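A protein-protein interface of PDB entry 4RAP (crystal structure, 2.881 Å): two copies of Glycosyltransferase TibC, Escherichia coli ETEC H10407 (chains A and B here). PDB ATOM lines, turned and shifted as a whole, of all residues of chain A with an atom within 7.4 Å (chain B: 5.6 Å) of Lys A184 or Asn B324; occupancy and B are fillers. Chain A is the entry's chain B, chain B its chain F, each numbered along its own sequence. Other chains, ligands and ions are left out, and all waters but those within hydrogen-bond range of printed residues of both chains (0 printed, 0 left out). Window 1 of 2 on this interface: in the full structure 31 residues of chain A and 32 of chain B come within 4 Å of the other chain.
O of Lys A184 sits at hydrogen-bond distance from ND2 of Asn B324 (2.9 Å).
ND2 of Asn A324 is in hydrogen-bond range of O of Lys B184.
The backbone carbonyl oxygen of Asp A344 is in hydrogen-bond range of the side-chain amino group of Lys B184 (2.9 Å).
The backbone carbonyl oxygen (O) of Thr A346 sits at hydrogen-bond distance from the guanidinium group (NH2) of Arg A183, at 3.5 Å.
O of Val A185 sits at hydrogen-bond distance from NH1 of Arg A189, 2.7 Å away.
The guanidinium group (NH2) of Arg A189 is in hydrogen-bond range of the backbone carbonyl oxygen (O) of Asn A324, at 2.9 Å.
The backbone carbonyl oxygen (O) of Val B185 sits at hydrogen-bond distance from the guanidinium group (NH1) of Arg B189, at 2.6 Å.
NH2 of Arg B189 is in hydrogen-bond range of O of Asn B324, 3.0 Å away.
OD2 of Asp B344 sits at hydrogen-bond distance from N of Leu B322, at 2.8 Å.
CA of Val A180 touches OH of Tyr B340 (3.2 Å).
Lys A184 touches Leu B322.
Asp B344 touches Lys A184 (O to NZ, 3.8 Å).
Lys A184 touches Asp B345 (NZ to CA, 3.7 Å).
ND2 of Asn B324 touches CA of Val A185, at 3.6 Å.
Tyr A193 touches Pro B323.
Asn A324 touches Val B185 (ND2 to CA, 3.7 Å).
Thr B346 touches Thr A346 (OG1 to OG1, 3.6 Å).
Printed residues of chain B within 4 Å of Val A180: Tyr B340 (3.2 Å).
Of chain B, only Leu B322 (3.7 Å), Asn B324 (2.9 Å), Asp B344 (3.8 Å) and Asp B345 (3.7 Å) come within 4 Å of Lys A184.
Of the printed residues of chain B, Thr A346 touches Thr B346.
Asn B324 touches just these residues of chain A: Lys A184 and Val A185.
Of the printed residues of chain A, Tyr B340 touches Val A180 (3.2 Å).
Of the printed residues of chain A, Asp B344 touches Lys A184.
Hydrophobic or aromatic side chains of chain B that line the printed part of chain A: Val B185, Leu B322, Pro B323 and Tyr B340.
Along chain B the printed residues that touch a printed residue of chain A span positions 184 to 346.
Of the 14 printed residues of chain A, 7 touch a printed residue of chain B.
Printed residues of chain A that touch a printed residue of chain B: Val A180, Lys A184, Val A185, Tyr A193, Asn A324, Asp A344 and Thr A346.
Hydrophobic or aromatic side chains of chain A within 4 Å of the printed part of chain B: Val A180, Val A185 and Tyr A193.
Among the printed residues, 11 pairs touch across the chains.
Lys A184 touches Asn B324, and with the chains exchanged Asn A324 touches Lys B184.
Lys A184 touches Asp B344, and with the chains exchanged Asp A344 touches Lys B184.
Val A185 touches Asn B324, and with the chains exchanged Asn A324 touches Val B185.
Thr B346 touches its own counterpart, Thr A346.
7 positions are printed for both chains.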
ATOM      1  N   VAL A 180     -26.091  16.625 -24.579  1.00  0.00           N
ATOM      2  CA  VAL A 180     -26.617  15.260 -24.560  1.00  0.00           C
ATOM      3  C   VAL A 180     -27.500  15.063 -23.316  1.00  0.00           C
ATOM      4  O   VAL A 180     -27.226  15.643 -22.255  1.00  0.00           O
ATOM      5  CB  VAL A 180     -25.450  14.257 -24.500  1.00  0.00           C
ATOM      6  CG1 VAL A 180     -25.952  12.837 -24.377  1.00  0.00           C
ATOM      7  CG2 VAL A 180     -24.563  14.413 -25.719  1.00  0.00           C
ATOM      8  N   ASP A 181     -28.548  14.252 -23.449  1.00  0.00           N
ATOM      9  CA  ASP A 181     -29.434  13.910 -22.327  1.00  0.00           C
ATOM     10  C   ASP A 181     -28.594  13.371 -21.162  1.00  0.00           C
ATOM     11  O   ASP A 181     -27.812  12.434 -21.334  1.00  0.00           O
ATOM     12  CB  ASP A 181     -30.445  12.867 -22.792  1.00  0.00           C
ATOM     13  CG  ASP A 181     -31.453  12.469 -21.703  1.00  0.00           C
ATOM     14  OD1 ASP A 181     -31.244  12.768 -20.492  1.00  0.00           O
ATOM     15  OD2 ASP A 181     -32.459  11.819 -22.077  1.00  0.00           O
ATOM     16  N   PHE A 182     -28.747  13.966 -19.981  1.00  0.00           N
ATOM     17  CA  PHE A 182     -27.876  13.622 -18.874  1.00  0.00           C
ATOM     18  C   PHE A 182     -27.963  12.148 -18.487  1.00  0.00           C
ATOM     19  O   PHE A 182     -27.030  11.587 -17.894  1.00  0.00           O
ATOM     20  CB  PHE A 182     -28.136  14.524 -17.665  1.00  0.00           C
ATOM     21  CG  PHE A 182     -29.409  14.219 -16.933  1.00  0.00           C
ATOM     22  CD1 PHE A 182     -29.463  13.209 -16.000  1.00  0.00           C
ATOM     23  CD2 PHE A 182     -30.533  14.980 -17.138  1.00  0.00           C
ATOM     24  CE1 PHE A 182     -30.636  12.934 -15.320  1.00  0.00           C
ATOM     25  CE2 PHE A 182     -31.708  14.726 -16.459  1.00  0.00           C
ATOM     26  CZ  PHE A 182     -31.761  13.702 -15.549  1.00  0.00           C
ATOM     27  N   ARG A 183     -29.086  11.524 -18.815  1.00  0.00           N
ATOM     28  CA  ARG A 183     -29.291  10.132 -18.480  1.00  0.00           C
ATOM     29  C   ARG A 183     -28.371   9.192 -19.260  1.00  0.00           C
ATOM     30  O   ARG A 183     -28.115   8.063 -18.831  1.00  0.00           O
ATOM     31  CB  ARG A 183     -30.744   9.758 -18.692  1.00  0.00           C
ATOM     32  CG  ARG A 183     -31.654  10.450 -17.703  1.00  0.00           C
ATOM     33  CD  ARG A 183     -33.118  10.204 -18.013  1.00  0.00           C
ATOM     34  NE  ARG A 183     -33.511  10.776 -19.301  1.00  0.00           N
ATOM     35  CZ  ARG A 183     -34.745  10.726 -19.781  1.00  0.00           C
ATOM     36  NH1 ARG A 183     -35.713  10.160 -19.071  1.00  0.00           N
ATOM     37  NH2 ARG A 183     -35.013  11.242 -20.960  1.00  0.00           N
ATOM     38  N   LYS A 184     -27.857   9.675 -20.385  1.00  0.00           N
ATOM     39  CA  LYS A 184     -26.979   8.888 -21.232  1.00  0.00           C
ATOM     40  C   LYS A 184     -25.511   8.958 -20.811  1.00  0.00           C
ATOM     41  O   LYS A 184     -24.733   8.055 -21.109  1.00  0.00           O
ATOM     42  CB  LYS A 184     -27.174   9.270 -22.707  1.00  0.00           C
ATOM     43  CG  LYS A 184     -28.561   8.889 -23.216  1.00  0.00           C
ATOM     44  CD  LYS A 184     -29.080   9.714 -24.404  1.00  0.00           C
ATOM     45  CE  LYS A 184     -28.784   9.098 -25.779  1.00  0.00           C
ATOM     46  NZ  LYS A 184     -29.286   7.703 -25.969  1.00  0.00           N
ATOM     47  N   VAL A 185     -25.157   9.968 -20.034  1.00  0.00           N
ATOM     48  CA  VAL A 185     -23.762  10.203 -19.678  1.00  0.00           C
ATOM     49  C   VAL A 185     -23.483  10.236 -18.191  1.00  0.00           C
ATOM     50  O   VAL A 185     -22.323  10.210 -17.785  1.00  0.00           O
ATOM     51  CB  VAL A 185     -23.282  11.537 -20.259  1.00  0.00           C
ATOM     52  CG1 VAL A 185     -23.200  11.443 -21.781  1.00  0.00           C
ATOM     53  CG2 VAL A 185     -24.218  12.668 -19.823  1.00  0.00           C
ATOM     54  N   GLY A 186     -24.546  10.305 -17.381  1.00  0.00           N
ATOM     55  CA  GLY A 186     -24.433  10.455 -15.910  1.00  0.00           C
ATOM     56  C   GLY A 186     -24.787  11.878 -15.484  1.00  0.00           C
ATOM     57  O   GLY A 186     -24.277  12.838 -16.061  1.00  0.00           O
ATOM     58  N   PHE A 187     -25.642  12.025 -14.468  1.00  0.00           N
ATOM     59  CA  PHE A 187     -26.137  13.359 -14.082  1.00  0.00           C
ATOM     60  C   PHE A 187     -25.005  14.335 -13.723  1.00  0.00           C
ATOM     61  O   PHE A 187     -25.089  15.518 -14.030  1.00  0.00           O
ATOM     62  CB  PHE A 187     -27.178  13.281 -12.950  1.00  0.00           C
ATOM     63  CG  PHE A 187     -26.577  13.211 -11.574  1.00  0.00           C
ATOM     64  CD1 PHE A 187     -26.173  11.993 -11.042  1.00  0.00           C
ATOM     65  CD2 PHE A 187     -26.409  14.368 -10.806  1.00  0.00           C
ATOM     66  CE1 PHE A 187     -25.616  11.931  -9.769  1.00  0.00           C
ATOM     67  CE2 PHE A 187     -25.840  14.307  -9.533  1.00  0.00           C
ATOM     68  CZ  PHE A 187     -25.446  13.090  -9.011  1.00  0.00           C
ATOM     69  N   ARG A 189     -21.604  14.039 -14.708  1.00  0.00           N
ATOM     70  CA  ARG A 189     -20.730  14.260 -15.871  1.00  0.00           C
ATOM     71  C   ARG A 189     -21.353  15.201 -16.882  1.00  0.00           C
ATOM     72  O   ARG A 189     -20.646  15.802 -17.666  1.00  0.00           O
ATOM     73  CB  ARG A 189     -20.365  12.942 -16.553  1.00  0.00           C
ATOM     74  CG  ARG A 189     -19.767  11.940 -15.609  1.00  0.00           C
ATOM     75  CD  ARG A 189     -19.304  10.695 -16.337  1.00  0.00           C
ATOM     76  NE  ARG A 189     -19.159   9.599 -15.391  1.00  0.00           N
ATOM     77  CZ  ARG A 189     -20.149   8.757 -15.074  1.00  0.00           C
ATOM     78  NH1 ARG A 189     -21.334   8.876 -15.658  1.00  0.00           N
ATOM     79  NH2 ARG A 189     -19.964   7.799 -14.173  1.00  0.00           N
ATOM     80  N   TYR A 193     -20.054  18.115 -20.011  1.00  0.00           N
ATOM     81  CA  TYR A 193     -20.524  18.243 -21.393  1.00  0.00           C
ATOM     82  C   TYR A 193     -21.071  19.638 -21.648  1.00  0.00           C
ATOM     83  O   TYR A 193     -20.751  20.263 -22.660  1.00  0.00           O
ATOM     84  CB  TYR A 193     -21.572  17.196 -21.730  1.00  0.00           C
ATOM     85  CG  TYR A 193     -21.007  15.811 -21.980  1.00  0.00           C
ATOM     86  CD1 TYR A 193     -20.713  14.959 -20.926  1.00  0.00           C
ATOM     87  CD2 TYR A 193     -20.832  15.337 -23.269  1.00  0.00           C
ATOM     88  CE1 TYR A 193     -20.212  13.690 -21.145  1.00  0.00           C
ATOM     89  CE2 TYR A 193     -20.347  14.069 -23.500  1.00  0.00           C
ATOM     90  CZ  TYR A 193     -20.037  13.249 -22.432  1.00  0.00           C
ATOM     91  OH  TYR A 193     -19.556  11.975 -22.661  1.00  0.00           O
ATOM     92  N   PRO A 199     -14.922  15.280 -19.443  1.00  0.00           N
ATOM     93  CA  PRO A 199     -16.126  14.905 -18.715  1.00  0.00           C
ATOM     94  C   PRO A 199     -15.883  13.890 -17.610  1.00  0.00           C
ATOM     95  O   PRO A 199     -16.823  13.445 -16.960  1.00  0.00           O
ATOM     96  CB  PRO A 199     -17.010  14.310 -19.805  1.00  0.00           C
ATOM     97  CG  PRO A 199     -16.034  13.716 -20.750  1.00  0.00           C
ATOM     98  CD  PRO A 199     -14.815  14.592 -20.732  1.00  0.00           C
ATOM     99  N   ASN A 324     -23.066   2.805 -13.285  1.00  0.00           N
ATOM    100  CA  ASN A 324     -22.329   3.953 -13.891  1.00  0.00           C
ATOM    101  C   ASN A 324     -22.991   5.336 -13.712  1.00  0.00           C
ATOM    102  O   ASN A 324     -22.481   6.343 -14.184  1.00  0.00           O
ATOM    103  CB  ASN A 324     -22.005   3.717 -15.373  1.00  0.00           C
ATOM    104  CG  ASN A 324     -23.253   3.520 -16.222  1.00  0.00           C
ATOM    105  OD1 ASN A 324     -24.367   3.446 -15.707  1.00  0.00           O
ATOM    106  ND2 ASN A 324     -23.066   3.400 -17.533  1.00  0.00           N
ATOM    107  N   ASP A 344     -32.266   6.084 -15.054  1.00  0.00           N
ATOM    108  CA  ASP A 344     -31.447   6.287 -16.242  1.00  0.00           C
ATOM    109  C   ASP A 344     -32.206   6.026 -17.527  1.00  0.00           C
ATOM    110  O   ASP A 344     -31.710   6.326 -18.599  1.00  0.00           O
ATOM    111  CB  ASP A 344     -30.218   5.385 -16.200  1.00  0.00           C
ATOM    112  CG  ASP A 344     -29.188   5.828 -15.156  1.00  0.00           C
ATOM    113  OD1 ASP A 344     -28.560   6.922 -15.321  1.00  0.00           O
ATOM    114  OD2 ASP A 344     -28.962   5.050 -14.201  1.00  0.00           O
ATOM    115  N   THR A 346     -34.380   6.492 -20.574  1.00  0.00           N
ATOM    116  CA  THR A 346     -34.807   7.633 -21.372  1.00  0.00           C
ATOM    117  C   THR A 346     -36.269   7.598 -21.846  1.00  0.00           C
ATOM    118  O   THR A 346     -36.791   8.596 -22.359  1.00  0.00           O
ATOM    119  CB  THR A 346     -33.894   7.861 -22.583  1.00  0.00           C
ATOM    120  OG1 THR A 346     -33.833   6.677 -23.358  1.00  0.00           O
ATOM    121  CG2 THR A 346     -32.511   8.229 -22.155  1.00  0.00           C
ATOM    122  N   LYS B 184     -26.501   0.969 -22.483  1.00  0.00           N
ATOM    123  CA  LYS B 184     -26.525   1.833 -21.305  1.00  0.00           C
ATOM    124  C   LYS B 184     -25.134   1.978 -20.699  1.00  0.00           C
ATOM    125  O   LYS B 184     -24.823   2.954 -20.024  1.00  0.00           O
ATOM    126  CB  LYS B 184     -27.474   1.266 -20.238  1.00  0.00           C
ATOM    127  CG  LYS B 184     -28.907   0.950 -20.683  1.00  0.00           C
ATOM    128  CD  LYS B 184     -29.647   2.211 -21.111  1.00  0.00           C
ATOM    129  CE  LYS B 184     -29.625   3.330 -20.058  1.00  0.00           C
ATOM    130  NZ  LYS B 184     -30.509   4.469 -20.456  1.00  0.00           N
ATOM    131  N   VAL B 185     -24.286   0.994 -20.948  1.00  0.00           N
ATOM    132  CA  VAL B 185     -22.990   0.936 -20.285  1.00  0.00           C
ATOM    133  C   VAL B 185     -21.810   1.008 -21.249  1.00  0.00           C
ATOM    134  O   VAL B 185     -20.683   1.238 -20.826  1.00  0.00           O
ATOM    135  CB  VAL B 185     -22.885  -0.347 -19.473  1.00  0.00           C
ATOM    136  CG1 VAL B 185     -23.898  -0.329 -18.327  1.00  0.00           C
ATOM    137  CG2 VAL B 185     -23.136  -1.544 -20.377  1.00  0.00           C
ATOM    138  N   GLY B 186     -22.082   0.830 -22.544  1.00  0.00           N
ATOM    139  CA  GLY B 186     -21.039   0.787 -23.580  1.00  0.00           C
ATOM    140  C   GLY B 186     -20.834  -0.648 -24.065  1.00  0.00           C
ATOM    141  O   GLY B 186     -20.747  -1.575 -23.251  1.00  0.00           O
ATOM    142  N   HIS B 188     -18.367  -2.383 -25.137  1.00  0.00           N
ATOM    143  CA  HIS B 188     -17.189  -3.101 -24.624  1.00  0.00           C
ATOM    144  C   HIS B 188     -17.279  -3.383 -23.152  1.00  0.00           C
ATOM    145  O   HIS B 188     -16.919  -4.465 -22.703  1.00  0.00           O
ATOM    146  CB  HIS B 188     -15.888  -2.363 -24.949  1.00  0.00           C
ATOM    147  CG  HIS B 188     -15.808  -0.955 -24.372  1.00  0.00           C
ATOM    148  ND1 HIS B 188     -16.638   0.035 -24.749  1.00  0.00           N
ATOM    149  CD2 HIS B 188     -14.926  -0.392 -23.451  1.00  0.00           C
ATOM    150  CE1 HIS B 188     -16.305   1.168 -24.105  1.00  0.00           C
ATOM    151  NE2 HIS B 188     -15.264   0.902 -23.307  1.00  0.00           N
ATOM    152  N   ARG B 189     -17.753  -2.411 -22.377  1.00  0.00           N
ATOM    153  CA  ARG B 189     -17.869  -2.585 -20.927  1.00  0.00           C
ATOM    154  C   ARG B 189     -18.887  -3.658 -20.561  1.00  0.00           C
ATOM    155  O   ARG B 189     -18.848  -4.205 -19.470  1.00  0.00           O
ATOM    156  CB  ARG B 189     -18.226  -1.261 -20.253  1.00  0.00           C
ATOM    157  CG  ARG B 189     -17.211  -0.183 -20.535  1.00  0.00           C
ATOM    158  CD  ARG B 189     -17.494   1.068 -19.733  1.00  0.00           C
ATOM    159  NE  ARG B 189     -16.845   2.202 -20.355  1.00  0.00           N
ATOM    160  CZ  ARG B 189     -17.407   2.943 -21.301  1.00  0.00           C
ATOM    161  NH1 ARG B 189     -18.641   2.671 -21.718  1.00  0.00           N
ATOM    162  NH2 ARG B 189     -16.730   3.932 -21.852  1.00  0.00           N
ATOM    163  N   LEU B 322     -22.312   8.039 -29.045  1.00  0.00           N
ATOM    164  CA  LEU B 322     -21.893   9.111 -28.097  1.00  0.00           C
ATOM    165  C   LEU B 322     -20.430   8.970 -27.699  1.00  0.00           C
ATOM    166  O   LEU B 322     -19.881   7.867 -27.727  1.00  0.00           O
ATOM    167  CB  LEU B 322     -22.760   9.096 -26.823  1.00  0.00           C
ATOM    168  CG  LEU B 322     -24.244   9.336 -27.046  1.00  0.00           C
ATOM    169  CD1 LEU B 322     -25.031   9.108 -25.770  1.00  0.00           C
ATOM    170  CD2 LEU B 322     -24.430  10.741 -27.570  1.00  0.00           C
ATOM    171  N   PRO B 323     -19.806  10.079 -27.280  1.00  0.00           N
ATOM    172  CA  PRO B 323     -18.405  10.012 -26.821  1.00  0.00           C
ATOM    173  C   PRO B 323     -18.126   8.860 -25.841  1.00  0.00           C
ATOM    174  O   PRO B 323     -17.126   8.181 -25.991  1.00  0.00           O
ATOM    175  CB  PRO B 323     -18.187  11.371 -26.149  1.00  0.00           C
ATOM    176  CG  PRO B 323     -19.130  12.278 -26.865  1.00  0.00           C
ATOM    177  CD  PRO B 323     -20.341  11.451 -27.243  1.00  0.00           C
ATOM    178  N   ASN B 324     -19.000   8.638 -24.860  1.00  0.00           N
ATOM    179  CA  ASN B 324     -18.746   7.611 -23.833  1.00  0.00           C
ATOM    180  C   ASN B 324     -18.953   6.162 -24.322  1.00  0.00           C
ATOM    181  O   ASN B 324     -18.795   5.206 -23.564  1.00  0.00           O
ATOM    182  CB  ASN B 324     -19.565   7.888 -22.544  1.00  0.00           C
ATOM    183  CG  ASN B 324     -21.090   7.848 -22.779  1.00  0.00           C
ATOM    184  OD1 ASN B 324     -21.556   7.764 -23.912  1.00  0.00           O
ATOM    185  ND2 ASN B 324     -21.864   7.914 -21.696  1.00  0.00           N
ATOM    186  N   SER B 325     -19.293   6.014 -25.596  1.00  0.00           N
ATOM    187  CA  SER B 325     -19.615   4.713 -26.151  1.00  0.00           C
ATOM    188  C   SER B 325     -18.347   3.897 -26.474  1.00  0.00           C
ATOM    189  O   SER B 325     -18.395   2.667 -26.596  1.00  0.00           O
ATOM    190  CB  SER B 325     -20.481   4.898 -27.389  1.00  0.00           C
ATOM    191  OG  SER B 325     -20.909   3.655 -27.886  1.00  0.00           O
ATOM    192  N   GLU B 326     -17.220   4.591 -26.629  1.00  0.00           N
ATOM    193  CA  GLU B 326     -15.934   3.941 -26.873  1.00  0.00           C
ATOM    194  C   GLU B 326     -14.964   4.324 -25.757  1.00  0.00           C
ATOM    195  O   GLU B 326     -15.366   4.947 -24.769  1.00  0.00           O
ATOM    196  CB  GLU B 326     -15.357   4.348 -28.233  1.00  0.00           C
ATOM    197  CG  GLU B 326     -16.222   3.997 -29.434  1.00  0.00           C
ATOM    198  CD  GLU B 326     -17.312   5.023 -29.712  1.00  0.00           C
ATOM    199  OE1 GLU B 326     -17.307   6.094 -29.069  1.00  0.00           O
ATOM    200  OE2 GLU B 326     -18.176   4.762 -30.582  1.00  0.00           O
ATOM    201  N   ARG B 332     -11.295  12.830 -29.064  1.00  0.00           N
ATOM    202  CA  ARG B 332     -12.580  12.376 -29.590  1.00  0.00           C
ATOM    203  C   ARG B 332     -13.272  13.555 -30.307  1.00  0.00           C
ATOM    204  O   ARG B 332     -13.295  14.661 -29.792  1.00  0.00           O
ATOM    205  CB  ARG B 332     -13.446  11.801 -28.446  1.00  0.00           C
ATOM    206  CG  ARG B 332     -14.913  11.583 -28.757  1.00  0.00           C
ATOM    207  CD  ARG B 332     -15.178  10.349 -29.603  1.00  0.00           C
ATOM    208  NE  ARG B 332     -16.480  10.517 -30.252  1.00  0.00           N
ATOM    209  CZ  ARG B 332     -17.371   9.546 -30.414  1.00  0.00           C
ATOM    210  NH1 ARG B 332     -18.536   9.812 -30.970  1.00  0.00           N
ATOM    211  NH2 ARG B 332     -17.112   8.318 -29.992  1.00  0.00           N
ATOM    212  N   TYR B 340     -27.475  12.732 -33.553  1.00  0.00           N
ATOM    213  CA  TYR B 340     -26.290  12.009 -33.116  1.00  0.00           C
ATOM    214  C   TYR B 340     -26.713  10.798 -32.277  1.00  0.00           C
ATOM    215  O   TYR B 340     -27.860  10.697 -31.869  1.00  0.00           O
ATOM    216  CB  TYR B 340     -25.365  12.904 -32.327  1.00  0.00           C
ATOM    217  CG  TYR B 340     -25.986  13.470 -31.093  1.00  0.00           C
ATOM    218  CD1 TYR B 340     -26.221  12.673 -29.985  1.00  0.00           C
ATOM    219  CD2 TYR B 340     -26.316  14.832 -31.022  1.00  0.00           C
ATOM    220  CE1 TYR B 340     -26.782  13.201 -28.836  1.00  0.00           C
ATOM    221  CE2 TYR B 340     -26.867  15.385 -29.878  1.00  0.00           C
ATOM    222  CZ  TYR B 340     -27.106  14.565 -28.782  1.00  0.00           C
ATOM    223  OH  TYR B 340     -27.660  15.091 -27.626  1.00  0.00           O
ATOM    224  N   GLY B 341     -25.809   9.846 -32.086  1.00  0.00           N
ATOM    225  CA  GLY B 341     -26.090   8.718 -31.206  1.00  0.00           C
ATOM    226  C   GLY B 341     -27.192   7.743 -31.571  1.00  0.00           C
ATOM    227  O   GLY B 341     -27.820   7.206 -30.694  1.00  0.00           O
ATOM    228  N   ASP B 344     -26.546   4.433 -29.549  1.00  0.00           N
ATOM    229  CA  ASP B 344     -26.757   4.315 -28.117  1.00  0.00           C
ATOM    230  C   ASP B 344     -28.216   4.392 -27.686  1.00  0.00           C
ATOM    231  O   ASP B 344     -28.542   4.025 -26.569  1.00  0.00           O
ATOM    232  CB  ASP B 344     -25.966   5.382 -27.400  1.00  0.00           C
ATOM    233  CG  ASP B 344     -24.492   5.073 -27.352  1.00  0.00           C
ATOM    234  OD1 ASP B 344     -24.074   4.093 -26.671  1.00  0.00           O
ATOM    235  OD2 ASP B 344     -23.741   5.823 -27.993  1.00  0.00           O
ATOM    236  N   ASP B 345     -29.089   4.836 -28.585  1.00  0.00           N
ATOM    237  CA  ASP B 345     -30.493   5.094 -28.266  1.00  0.00           C
ATOM    238  C   ASP B 345     -31.308   3.803 -28.056  1.00  0.00           C
ATOM    239  O   ASP B 345     -31.507   3.015 -28.992  1.00  0.00           O
ATOM    240  CB  ASP B 345     -31.102   5.960 -29.369  1.00  0.00           C
ATOM    241  CG  ASP B 345     -32.495   6.480 -29.025  1.00  0.00           C
ATOM    242  OD1 ASP B 345     -33.215   5.851 -28.217  1.00  0.00           O
ATOM    243  OD2 ASP B 345     -32.881   7.522 -29.594  1.00  0.00           O
ATOM    244  N   THR B 346     -31.784   3.598 -26.832  1.00  0.00           N
ATOM    245  CA  THR B 346     -32.507   2.370 -26.489  1.00  0.00           C
ATOM    246  C   THR B 346     -33.908   2.251 -27.086  1.00  0.00           C
ATOM    247  O   THR B 346     -34.521   1.186 -27.022  1.00  0.00           O
ATOM    248  CB  THR B 346     -32.590   2.159 -24.967  1.00  0.00           C
ATOM    249  OG1 THR B 346     -33.183   3.302 -24.355  1.00  0.00           O
ATOM    250  CG2 THR B 346     -31.203   1.931 -24.386  1.00  0.00           C
